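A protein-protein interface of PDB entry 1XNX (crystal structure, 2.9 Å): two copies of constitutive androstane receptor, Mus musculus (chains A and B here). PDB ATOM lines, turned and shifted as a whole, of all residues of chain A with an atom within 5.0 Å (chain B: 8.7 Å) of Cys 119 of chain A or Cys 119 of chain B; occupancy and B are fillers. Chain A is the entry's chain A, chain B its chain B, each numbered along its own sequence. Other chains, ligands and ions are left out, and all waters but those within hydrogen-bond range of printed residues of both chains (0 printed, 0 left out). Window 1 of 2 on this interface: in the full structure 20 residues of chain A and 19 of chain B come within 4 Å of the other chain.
Cys 119 of chain A touches one residue of chain B.
Cys 119 of chain B touches just one residue of chain A: Cys 119 (2.8 Å).
Phe 118 of chain A touches one residue of chain B.
Of the printed residues of chain B, Thr 117 of chain A touches Gln 121.
Printed residues of chain A within 4 Å of Phe 118 of chain B: Gln 121 (3.9996 Å).
Of the printed residues of chain B, Phe 126 of chain A touches Thr 122 and Phe 126.
Lys 155 of chain B touches none of the printed residues of chain A.
Gly 159 of chain B touches none of the printed residues of chain A.
The nearest residue of chain A that does not touch Cys 119 of chain B is Gln 121 of chain A (4.2 Å).
The side-chain hydroxyl (OG1) of Thr 122 of chain B is in hydrogen-bond range of the side-chain sulfur (SG) of Cys 119 of chain B (3.4 Å).
N of Thr 122 of chain A lies within hydrogen-bond range of SG of Cys 119 of chain A.
O of Phe 118 of chain B sits close to NZ of Lys 158 of chain B (2.9 Å).
The side-chain sulfur (SG) of Cys 119 of chain B sits close to the backbone NH (N) of Gln 121 of chain B (3.4 Å).
The side-chain amide nitrogen of Asn 124 of chain A sits at hydrogen-bond distance from the backbone carbonyl oxygen of Thr 122 of chain A (3.3 Å).
The side-chain sulfur (SG) of Cys 119 of chain A lies close to the backbone NH (N) of Gln 121 of chain A (3.6 Å).
The side-chain amide nitrogen (NE2) of Gln 121 of chain A is in hydrogen-bond range of the backbone carbonyl oxygen (O) of Thr 116 of chain B (3.1 Å).
The side-chain amide oxygen (OE1) of Gln 121 of chain A sits at hydrogen-bond distance from the side-chain amino group (NZ) of Lys 158 of chain B (2.9 Å).
The side-chain sulfur (SG) of Cys 119 of chain B sits close to the side-chain sulfur (SG) of Cys 119 of chain A (2.8 Å).
Printed residues of chain A that touch a printed residue of chain B: Thr 117, Phe 118, Cys 119, Gln 121, Thr 122 and Phe 126.
Hydrophobic or aromatic side chains of chain A that line the printed part of chain B: Phe 126.
Along chain A the printed residues that touch a printed residue of chain B span positions 117 to 126.
Printed residues of chain B that touch a printed residue of chain A: Thr 116, Phe 118, Cys 119, Gln 121, Thr 122, Phe 126 and Lys 158.
Hydrophobic or aromatic side chains of chain B within 4 Å of the printed part of chain A: Phe 126.
Among the printed residues, 9 pairs touch across the chains.
Phe 118 of chain A touches Gln 121 of chain B, and with the chains exchanged Gln 121 of chain A touches Phe 118 of chain B.
Cys 119 of chain A touches its own counterpart, Cys 119 of chain B.
Thr 122 of chain A touches Phe 126 of chain B, and with the chains exchanged Phe 126 of chain A touches Thr 122 of chain B.
Phe 126 of chain A touches its own counterpart, Phe 126 of chain B.
Of the 9 pairs that touch across the chains among the printed residues, 6 have their exchanged pair printed and touching as well.
Among the printed residues, merely in contact across the chains: Thr 117 of chain A with Gln 121 of chain B, Phe 118 of chain A with Gln 121 of chain B, Gln 121 of chain A with Phe 118 of chain B, Thr 122 of chain A with Phe 126 of chain B, Phe 126 of chain A with Thr 122 of chain B and Phe 126 of chain A with Phe 126 of chain B.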
ATOM      1  N   THR A 117       1.282 -35.140   7.632  1.00  0.00           N
ATOM      2  CA  THR A 117       0.562 -34.008   7.064  1.00  0.00           C
ATOM      3  C   THR A 117      -0.929 -34.287   7.071  1.00  0.00           C
ATOM      4  O   THR A 117      -1.710 -33.488   6.561  1.00  0.00           O
ATOM      5  CB  THR A 117       0.972 -33.755   5.589  1.00  0.00           C
ATOM      6  OG1 THR A 117       0.459 -34.817   4.770  1.00  0.00           O
ATOM      7  CG2 THR A 117       2.494 -33.703   5.439  1.00  0.00           C
ATOM      8  N   PHE A 118      -1.324 -35.416   7.649  1.00  0.00           N
ATOM      9  CA  PHE A 118      -2.730 -35.806   7.675  1.00  0.00           C
ATOM     10  C   PHE A 118      -3.556 -35.125   8.752  1.00  0.00           C
ATOM     11  O   PHE A 118      -3.147 -35.050   9.896  1.00  0.00           O
ATOM     12  CB  PHE A 118      -2.849 -37.327   7.843  1.00  0.00           C
ATOM     13  CG  PHE A 118      -4.260 -37.852   7.725  1.00  0.00           C
ATOM     14  CD1 PHE A 118      -4.903 -37.885   6.490  1.00  0.00           C
ATOM     15  CD2 PHE A 118      -4.945 -38.308   8.854  1.00  0.00           C
ATOM     16  CE1 PHE A 118      -6.208 -38.365   6.385  1.00  0.00           C
ATOM     17  CE2 PHE A 118      -6.248 -38.788   8.760  1.00  0.00           C
ATOM     18  CZ  PHE A 118      -6.881 -38.818   7.526  1.00  0.00           C
ATOM     19  N   CYS A 119      -4.728 -34.633   8.363  1.00  0.00           N
ATOM     20  CA  CYS A 119      -5.658 -33.976   9.274  1.00  0.00           C
ATOM     21  C   CYS A 119      -6.794 -34.955   9.621  1.00  0.00           C
ATOM     22  O   CYS A 119      -7.469 -35.466   8.729  1.00  0.00           O
ATOM     23  CB  CYS A 119      -6.230 -32.714   8.611  1.00  0.00           C
ATOM     24  SG  CYS A 119      -7.713 -32.009   9.417  1.00  0.00           S
ATOM     25  N   LEU A 120      -7.000 -35.215  10.912  1.00  0.00           N
ATOM     26  CA  LEU A 120      -8.042 -36.145  11.345  1.00  0.00           C
ATOM     27  C   LEU A 120      -9.439 -35.592  11.128  1.00  0.00           C
ATOM     28  O   LEU A 120     -10.362 -36.316  10.746  1.00  0.00           O
ATOM     29  CB  LEU A 120      -7.874 -36.482  12.828  1.00  0.00           C
ATOM     30  CG  LEU A 120      -7.810 -37.974  13.183  1.00  0.00           C
ATOM     31  CD1 LEU A 120      -7.817 -38.155  14.692  1.00  0.00           C
ATOM     32  CD2 LEU A 120      -8.985 -38.690  12.552  1.00  0.00           C
ATOM     33  N   GLN A 121      -9.590 -34.299  11.384  1.00  0.00           N
ATOM     34  CA  GLN A 121     -10.865 -33.606  11.238  1.00  0.00           C
ATOM     35  C   GLN A 121     -11.435 -33.629   9.813  1.00  0.00           C
ATOM     36  O   GLN A 121     -12.647 -33.709   9.631  1.00  0.00           O
ATOM     37  CB  GLN A 121     -10.696 -32.153  11.687  1.00  0.00           C
ATOM     38  CG  GLN A 121     -11.965 -31.323  11.648  1.00  0.00           C
ATOM     39  CD  GLN A 121     -13.072 -31.942  12.463  1.00  0.00           C
ATOM     40  OE1 GLN A 121     -12.828 -32.547  13.510  1.00  0.00           O
ATOM     41  NE2 GLN A 121     -14.303 -31.789  11.993  1.00  0.00           N
ATOM     42  N   THR A 122     -10.575 -33.566   8.804  1.00  0.00           N
ATOM     43  CA  THR A 122     -11.070 -33.546   7.439  1.00  0.00           C
ATOM     44  C   THR A 122     -10.579 -34.697   6.543  1.00  0.00           C
ATOM     45  O   THR A 122     -10.963 -34.795   5.373  1.00  0.00           O
ATOM     46  CB  THR A 122     -10.705 -32.212   6.795  1.00  0.00           C
ATOM     47  OG1 THR A 122      -9.300 -32.184   6.509  1.00  0.00           O
ATOM     48  CG2 THR A 122     -11.030 -31.088   7.737  1.00  0.00           C
ATOM     49  N   GLU A 123      -9.734 -35.563   7.095  1.00  0.00           N
ATOM     50  CA  GLU A 123      -9.193 -36.689   6.348  1.00  0.00           C
ATOM     51  C   GLU A 123      -8.592 -36.233   5.020  1.00  0.00           C
ATOM     52  O   GLU A 123      -8.929 -36.756   3.943  1.00  0.00           O
ATOM     53  CB  GLU A 123     -10.291 -37.707   6.100  1.00  0.00           C
ATOM     54  CG  GLU A 123     -11.176 -37.913   7.303  1.00  0.00           C
ATOM     55  CD  GLU A 123     -12.275 -38.887   7.023  1.00  0.00           C
ATOM     56  OE1 GLU A 123     -12.962 -38.703   5.995  1.00  0.00           O
ATOM     57  OE2 GLU A 123     -12.445 -39.829   7.828  1.00  0.00           O
ATOM     58  N   ASN A 124      -7.714 -35.237   5.108  1.00  0.00           N
ATOM     59  CA  ASN A 124      -7.023 -34.705   3.947  1.00  0.00           C
ATOM     60  C   ASN A 124      -5.579 -34.472   4.337  1.00  0.00           C
ATOM     61  O   ASN A 124      -5.294 -34.198   5.504  1.00  0.00           O
ATOM     62  CB  ASN A 124      -7.643 -33.385   3.505  1.00  0.00           C
ATOM     63  CG  ASN A 124      -9.027 -33.561   2.934  1.00  0.00           C
ATOM     64  OD1 ASN A 124      -9.325 -34.577   2.313  1.00  0.00           O
ATOM     65  ND2 ASN A 124      -9.876 -32.563   3.125  1.00  0.00           N
ATOM     66  N   PHE A 125      -4.667 -34.597   3.375  1.00  0.00           N
ATOM     67  CA  PHE A 125      -3.256 -34.365   3.649  1.00  0.00           C
ATOM     68  C   PHE A 125      -2.940 -32.950   3.193  1.00  0.00           C
ATOM     69  O   PHE A 125      -3.300 -32.565   2.081  1.00  0.00           O
ATOM     70  CB  PHE A 125      -2.368 -35.350   2.878  1.00  0.00           C
ATOM     71  CG  PHE A 125      -2.566 -36.800   3.256  1.00  0.00           C
ATOM     72  CD1 PHE A 125      -3.697 -37.499   2.850  1.00  0.00           C
ATOM     73  CD2 PHE A 125      -1.601 -37.476   4.001  1.00  0.00           C
ATOM     74  CE1 PHE A 125      -3.862 -38.852   3.179  1.00  0.00           C
ATOM     75  CE2 PHE A 125      -1.755 -38.820   4.333  1.00  0.00           C
ATOM     76  CZ  PHE A 125      -2.890 -39.509   3.918  1.00  0.00           C
ATOM     77  N   PHE A 126      -2.296 -32.167   4.053  1.00  0.00           N
ATOM     78  CA  PHE A 126      -1.922 -30.799   3.697  1.00  0.00           C
ATOM     79  C   PHE A 126      -0.428 -30.736   3.434  1.00  0.00           C
ATOM     80  O   PHE A 126       0.382 -30.682   4.374  1.00  0.00           O
ATOM     81  CB  PHE A 126      -2.293 -29.820   4.806  1.00  0.00           C
ATOM     82  CG  PHE A 126      -3.771 -29.611   4.949  1.00  0.00           C
ATOM     83  CD1 PHE A 126      -4.563 -30.563   5.572  1.00  0.00           C
ATOM     84  CD2 PHE A 126      -4.383 -28.485   4.403  1.00  0.00           C
ATOM     85  CE1 PHE A 126      -5.954 -30.395   5.647  1.00  0.00           C
ATOM     86  CE2 PHE A 126      -5.761 -28.315   4.474  1.00  0.00           C
ATOM     87  CZ  PHE A 126      -6.551 -29.269   5.096  1.00  0.00           C
ATOM     88  N   LEU B 114     -17.117 -24.215  18.874  1.00  0.00           N
ATOM     89  CA  LEU B 114     -16.242 -23.852  17.777  1.00  0.00           C
ATOM     90  C   LEU B 114     -15.173 -24.931  17.597  1.00  0.00           C
ATOM     91  O   LEU B 114     -14.742 -25.226  16.479  1.00  0.00           O
ATOM     92  CB  LEU B 114     -15.571 -22.512  18.076  1.00  0.00           C
ATOM     93  CG  LEU B 114     -15.292 -21.508  16.944  1.00  0.00           C
ATOM     94  CD1 LEU B 114     -14.285 -20.474  17.457  1.00  0.00           C
ATOM     95  CD2 LEU B 114     -14.741 -22.205  15.715  1.00  0.00           C
ATOM     96  N   ASN B 115     -14.757 -25.530  18.706  1.00  0.00           N
ATOM     97  CA  ASN B 115     -13.714 -26.554  18.687  1.00  0.00           C
ATOM     98  C   ASN B 115     -13.930 -27.725  17.730  1.00  0.00           C
ATOM     99  O   ASN B 115     -12.966 -28.391  17.346  1.00  0.00           O
ATOM    100  CB  ASN B 115     -13.496 -27.101  20.096  1.00  0.00           C
ATOM    101  CG  ASN B 115     -12.254 -27.952  20.200  1.00  0.00           C
ATOM    102  OD1 ASN B 115     -11.138 -27.452  20.060  1.00  0.00           O
ATOM    103  ND2 ASN B 115     -12.435 -29.245  20.443  1.00  0.00           N
ATOM    104  N   THR B 116     -15.178 -27.983  17.346  1.00  0.00           N
ATOM    105  CA  THR B 116     -15.464 -29.101  16.448  1.00  0.00           C
ATOM    106  C   THR B 116     -15.046 -28.826  15.009  1.00  0.00           C
ATOM    107  O   THR B 116     -15.089 -29.719  14.163  1.00  0.00           O
ATOM    108  CB  THR B 116     -16.962 -29.462  16.441  1.00  0.00           C
ATOM    109  OG1 THR B 116     -17.697 -28.433  15.763  1.00  0.00           O
ATOM    110  CG2 THR B 116     -17.483 -29.623  17.874  1.00  0.00           C
ATOM    111  N   THR B 117     -14.646 -27.587  14.739  1.00  0.00           N
ATOM    112  CA  THR B 117     -14.217 -27.192  13.406  1.00  0.00           C
ATOM    113  C   THR B 117     -12.707 -27.018  13.402  1.00  0.00           C
ATOM    114  O   THR B 117     -12.106 -26.678  12.380  1.00  0.00           O
ATOM    115  CB  THR B 117     -14.837 -25.856  12.999  1.00  0.00           C
ATOM    116  OG1 THR B 117     -14.311 -24.824  13.842  1.00  0.00           O
ATOM    117  CG2 THR B 117     -16.347 -25.893  13.142  1.00  0.00           C
ATOM    118  N   PHE B 118     -12.095 -27.252  14.557  1.00  0.00           N
ATOM    119  CA  PHE B 118     -10.653 -27.101  14.700  1.00  0.00           C
ATOM    120  C   PHE B 118      -9.874 -28.331  14.269  1.00  0.00           C
ATOM    121  O   PHE B 118     -10.176 -29.444  14.692  1.00  0.00           O
ATOM    122  CB  PHE B 118     -10.300 -26.780  16.151  1.00  0.00           C
ATOM    123  CG  PHE B 118      -8.852 -26.458  16.363  1.00  0.00           C
ATOM    124  CD1 PHE B 118      -8.252 -25.411  15.665  1.00  0.00           C
ATOM    125  CD2 PHE B 118      -8.086 -27.180  17.278  1.00  0.00           C
ATOM    126  CE1 PHE B 118      -6.905 -25.087  15.879  1.00  0.00           C
ATOM    127  CE2 PHE B 118      -6.735 -26.864  17.501  1.00  0.00           C
ATOM    128  CZ  PHE B 118      -6.146 -25.818  16.802  1.00  0.00           C
ATOM    129  N   CYS B 119      -8.882 -28.127  13.412  1.00  0.00           N
ATOM    130  CA  CYS B 119      -8.027 -29.214  12.969  1.00  0.00           C
ATOM    131  C   CYS B 119      -6.723 -29.003  13.726  1.00  0.00           C
ATOM    132  O   CYS B 119      -6.103 -27.956  13.604  1.00  0.00           O
ATOM    133  CB  CYS B 119      -7.785 -29.141  11.459  1.00  0.00           C
ATOM    134  SG  CYS B 119      -6.321 -30.074  10.912  1.00  0.00           S
ATOM    135  N   LEU B 120      -6.325 -29.995  14.516  1.00  0.00           N
ATOM    136  CA  LEU B 120      -5.111 -29.909  15.325  1.00  0.00           C
ATOM    137  C   LEU B 120      -3.817 -29.866  14.523  1.00  0.00           C
ATOM    138  O   LEU B 120      -2.805 -29.364  15.001  1.00  0.00           O
ATOM    139  CB  LEU B 120      -5.069 -31.080  16.312  1.00  0.00           C
ATOM    140  CG  LEU B 120      -3.947 -31.144  17.353  1.00  0.00           C
ATOM    141  CD1 LEU B 120      -3.856 -29.834  18.107  1.00  0.00           C
ATOM    142  CD2 LEU B 120      -4.226 -32.289  18.324  1.00  0.00           C
ATOM    143  N   GLN B 121      -3.857 -30.364  13.295  1.00  0.00           N
ATOM    144  CA  GLN B 121      -2.663 -30.397  12.456  1.00  0.00           C
ATOM    145  C   GLN B 121      -2.263 -29.034  11.901  1.00  0.00           C
ATOM    146  O   GLN B 121      -1.124 -28.584  12.069  1.00  0.00           O
ATOM    147  CB  GLN B 121      -2.871 -31.374  11.293  1.00  0.00           C
ATOM    148  CG  GLN B 121      -1.733 -32.351  11.106  1.00  0.00           C
ATOM    149  CD  GLN B 121      -0.456 -31.689  10.631  1.00  0.00           C
ATOM    150  OE1 GLN B 121       0.599 -32.314  10.600  1.00  0.00           O
ATOM    151  NE2 GLN B 121      -0.547 -30.425  10.252  1.00  0.00           N
ATOM    152  N   THR B 122      -3.208 -28.386  11.234  1.00  0.00           N
ATOM    153  CA  THR B 122      -2.962 -27.093  10.625  1.00  0.00           C
ATOM    154  C   THR B 122      -3.287 -25.909  11.540  1.00  0.00           C
ATOM    155  O   THR B 122      -2.907 -24.772  11.254  1.00  0.00           O
ATOM    156  CB  THR B 122      -3.785 -26.979   9.334  1.00  0.00           C
ATOM    157  OG1 THR B 122      -5.179 -27.125   9.642  1.00  0.00           O
ATOM    158  CG2 THR B 122      -3.387 -28.075   8.364  1.00  0.00           C
ATOM    159  N   GLU B 123      -3.984 -26.187  12.638  1.00  0.00           N
ATOM    160  CA  GLU B 123      -4.388 -25.162  13.588  1.00  0.00           C
ATOM    161  C   GLU B 123      -5.414 -24.181  13.005  1.00  0.00           C
ATOM    162  O   GLU B 123      -5.657 -23.109  13.565  1.00  0.00           O
ATOM    163  CB  GLU B 123      -3.168 -24.404  14.096  1.00  0.00           C
ATOM    164  CG  GLU B 123      -2.583 -24.999  15.362  1.00  0.00           C
ATOM    165  CD  GLU B 123      -1.300 -24.317  15.800  1.00  0.00           C
ATOM    166  OE1 GLU B 123      -1.275 -23.072  15.882  1.00  0.00           O
ATOM    167  OE2 GLU B 123      -0.318 -25.035  16.073  1.00  0.00           O
ATOM    168  N   ASN B 124      -6.015 -24.543  11.876  1.00  0.00           N
ATOM    169  CA  ASN B 124      -7.019 -23.687  11.263  1.00  0.00           C
ATOM    170  C   ASN B 124      -8.404 -24.097  11.743  1.00  0.00           C
ATOM    171  O   ASN B 124      -8.574 -25.142  12.371  1.00  0.00           O
ATOM    172  CB  ASN B 124      -6.986 -23.818   9.734  1.00  0.00           C
ATOM    173  CG  ASN B 124      -5.697 -23.300   9.121  1.00  0.00           C
ATOM    174  OD1 ASN B 124      -5.298 -22.159   9.359  1.00  0.00           O
ATOM    175  ND2 ASN B 124      -5.046 -24.137   8.312  1.00  0.00           N
ATOM    176  N   PHE B 125      -9.394 -23.260  11.461  1.00  0.00           N
ATOM    177  CA  PHE B 125     -10.768 -23.585  11.803  1.00  0.00           C
ATOM    178  C   PHE B 125     -11.486 -23.637  10.463  1.00  0.00           C
ATOM    179  O   PHE B 125     -11.482 -22.656   9.711  1.00  0.00           O
ATOM    180  CB  PHE B 125     -11.408 -22.515  12.694  1.00  0.00           C
ATOM    181  CG  PHE B 125     -10.903 -22.514  14.109  1.00  0.00           C
ATOM    182  CD1 PHE B 125      -9.721 -21.850  14.442  1.00  0.00           C
ATOM    183  CD2 PHE B 125     -11.608 -23.175  15.114  1.00  0.00           C
ATOM    184  CE1 PHE B 125      -9.247 -21.842  15.751  1.00  0.00           C
ATOM    185  CE2 PHE B 125     -11.138 -23.171  16.429  1.00  0.00           C
ATOM    186  CZ  PHE B 125      -9.951 -22.498  16.745  1.00  0.00           C
ATOM    187  N   PHE B 126     -12.079 -24.783  10.154  1.00  0.00           N
ATOM    188  CA  PHE B 126     -12.786 -24.937   8.893  1.00  0.00           C
ATOM    189  C   PHE B 126     -14.294 -24.791   9.076  1.00  0.00           C
ATOM    190  O   PHE B 126     -14.971 -25.707   9.528  1.00  0.00           O
ATOM    191  CB  PHE B 126     -12.448 -26.296   8.265  1.00  0.00           C
ATOM    192  CG  PHE B 126     -10.991 -26.454   7.915  1.00  0.00           C
ATOM    193  CD1 PHE B 126     -10.224 -27.463   8.494  1.00  0.00           C
ATOM    194  CD2 PHE B 126     -10.378 -25.581   7.017  1.00  0.00           C
ATOM    195  CE1 PHE B 126      -8.873 -27.596   8.187  1.00  0.00           C
ATOM    196  CE2 PHE B 126      -9.022 -25.705   6.701  1.00  0.00           C
ATOM    197  CZ  PHE B 126      -8.269 -26.711   7.286  1.00  0.00           C
ATOM    198  N   CYS B 131     -11.685 -20.742   6.002  1.00  0.00           N
ATOM    199  CA  CYS B 131     -10.526 -21.203   6.769  1.00  0.00           C
ATOM    200  C   CYS B 131     -10.002 -20.084   7.679  1.00  0.00           C
ATOM    201  O   CYS B 131      -9.318 -19.173   7.211  1.00  0.00           O
ATOM    202  CB  CYS B 131      -9.403 -21.648   5.826  1.00  0.00           C
ATOM    203  SG  CYS B 131      -7.877 -22.224   6.655  1.00  0.00           S
ATOM    204  N   TYR B 132     -10.309 -20.143   8.971  1.00  0.00           N
ATOM    205  CA  TYR B 132      -9.835 -19.106   9.887  1.00  0.00           C
ATOM    206  C   TYR B 132      -8.515 -19.472  10.571  1.00  0.00           C
ATOM    207  O   TYR B 132      -8.315 -20.607  11.011  1.00  0.00           O
ATOM    208  CB  TYR B 132     -10.880 -18.799  10.963  1.00  0.00           C
ATOM    209  CG  TYR B 132     -12.228 -18.352  10.442  1.00  0.00           C
ATOM    210  CD1 TYR B 132     -13.174 -19.283  10.014  1.00  0.00           C
ATOM    211  CD2 TYR B 132     -12.577 -17.002  10.423  1.00  0.00           C
ATOM    212  CE1 TYR B 132     -14.432 -18.880   9.591  1.00  0.00           C
ATOM    213  CE2 TYR B 132     -13.835 -16.588  10.000  1.00  0.00           C
ATOM    214  CZ  TYR B 132     -14.755 -17.529   9.588  1.00  0.00           C
ATOM    215  OH  TYR B 132     -16.000 -17.123   9.176  1.00  0.00           O
ATOM    216  N   LEU B 151      -5.719 -20.291  21.510  1.00  0.00           N
ATOM    217  CA  LEU B 151      -5.079 -21.362  20.771  1.00  0.00           C
ATOM    218  C   LEU B 151      -4.757 -22.524  21.702  1.00  0.00           C
ATOM    219  O   LEU B 151      -4.996 -23.688  21.361  1.00  0.00           O
ATOM    220  CB  LEU B 151      -3.799 -20.854  20.110  1.00  0.00           C
ATOM    221  CG  LEU B 151      -2.986 -21.835  19.253  1.00  0.00           C
ATOM    222  CD1 LEU B 151      -3.871 -22.410  18.139  1.00  0.00           C
ATOM    223  CD2 LEU B 151      -1.762 -21.121  18.670  1.00  0.00           C
ATOM    224  N   HIS B 154      -7.927 -24.521  22.508  1.00  0.00           N
ATOM    225  CA  HIS B 154      -8.311 -25.357  21.382  1.00  0.00           C
ATOM    226  C   HIS B 154      -7.338 -26.496  21.058  1.00  0.00           C
ATOM    227  O   HIS B 154      -7.762 -27.540  20.558  1.00  0.00           O
ATOM    228  CB  HIS B 154      -8.554 -24.472  20.148  1.00  0.00           C
ATOM    229  CG  HIS B 154      -9.809 -23.658  20.231  1.00  0.00           C
ATOM    230  ND1 HIS B 154     -11.055 -24.178  19.946  1.00  0.00           N
ATOM    231  CD2 HIS B 154     -10.021 -22.382  20.634  1.00  0.00           C
ATOM    232  CE1 HIS B 154     -11.977 -23.261  20.176  1.00  0.00           C
ATOM    233  NE2 HIS B 154     -11.377 -22.162  20.596  1.00  0.00           N
ATOM    234  N   LYS B 155      -6.046 -26.323  21.330  1.00  0.00           N
ATOM    235  CA  LYS B 155      -5.116 -27.421  21.056  1.00  0.00           C
ATOM    236  C   LYS B 155      -5.371 -28.485  22.124  1.00  0.00           C
ATOM    237  O   LYS B 155      -5.607 -29.650  21.808  1.00  0.00           O
ATOM    238  CB  LYS B 155      -3.642 -26.966  21.096  1.00  0.00           C
ATOM    239  CG  LYS B 155      -3.314 -25.800  20.154  1.00  0.00           C
ATOM    240  CD  LYS B 155      -2.165 -26.091  19.192  1.00  0.00           C
ATOM    241  CE  LYS B 155      -0.846 -26.262  19.920  1.00  0.00           C
ATOM    242  NZ  LYS B 155       0.332 -26.360  18.989  1.00  0.00           N
ATOM    243  N   LYS B 158      -8.986 -30.206  21.833  1.00  0.00           N
ATOM    244  CA  LYS B 158      -9.050 -31.032  20.634  1.00  0.00           C
ATOM    245  C   LYS B 158      -8.301 -32.345  20.821  1.00  0.00           C
ATOM    246  O   LYS B 158      -8.722 -33.378  20.312  1.00  0.00           O
ATOM    247  CB  LYS B 158      -8.459 -30.276  19.445  1.00  0.00           C
ATOM    248  CG  LYS B 158      -8.637 -30.985  18.125  1.00  0.00           C
ATOM    249  CD  LYS B 158     -10.093 -30.992  17.726  1.00  0.00           C
ATOM    250  CE  LYS B 158     -10.296 -31.679  16.395  1.00  0.00           C
ATOM    251  NZ  LYS B 158     -11.699 -31.530  15.935  1.00  0.00           N
ATOM    252  N   GLY B 159      -7.197 -32.296  21.563  1.00  0.00           N
ATOM    253  CA  GLY B 159      -6.393 -33.487  21.772  1.00  0.00           C
ATOM    254  C   GLY B 159      -6.994 -34.568  22.647  1.00  0.00           C
ATOM    255  O   GLY B 159      -6.326 -35.547  22.978  1.00  0.00           O
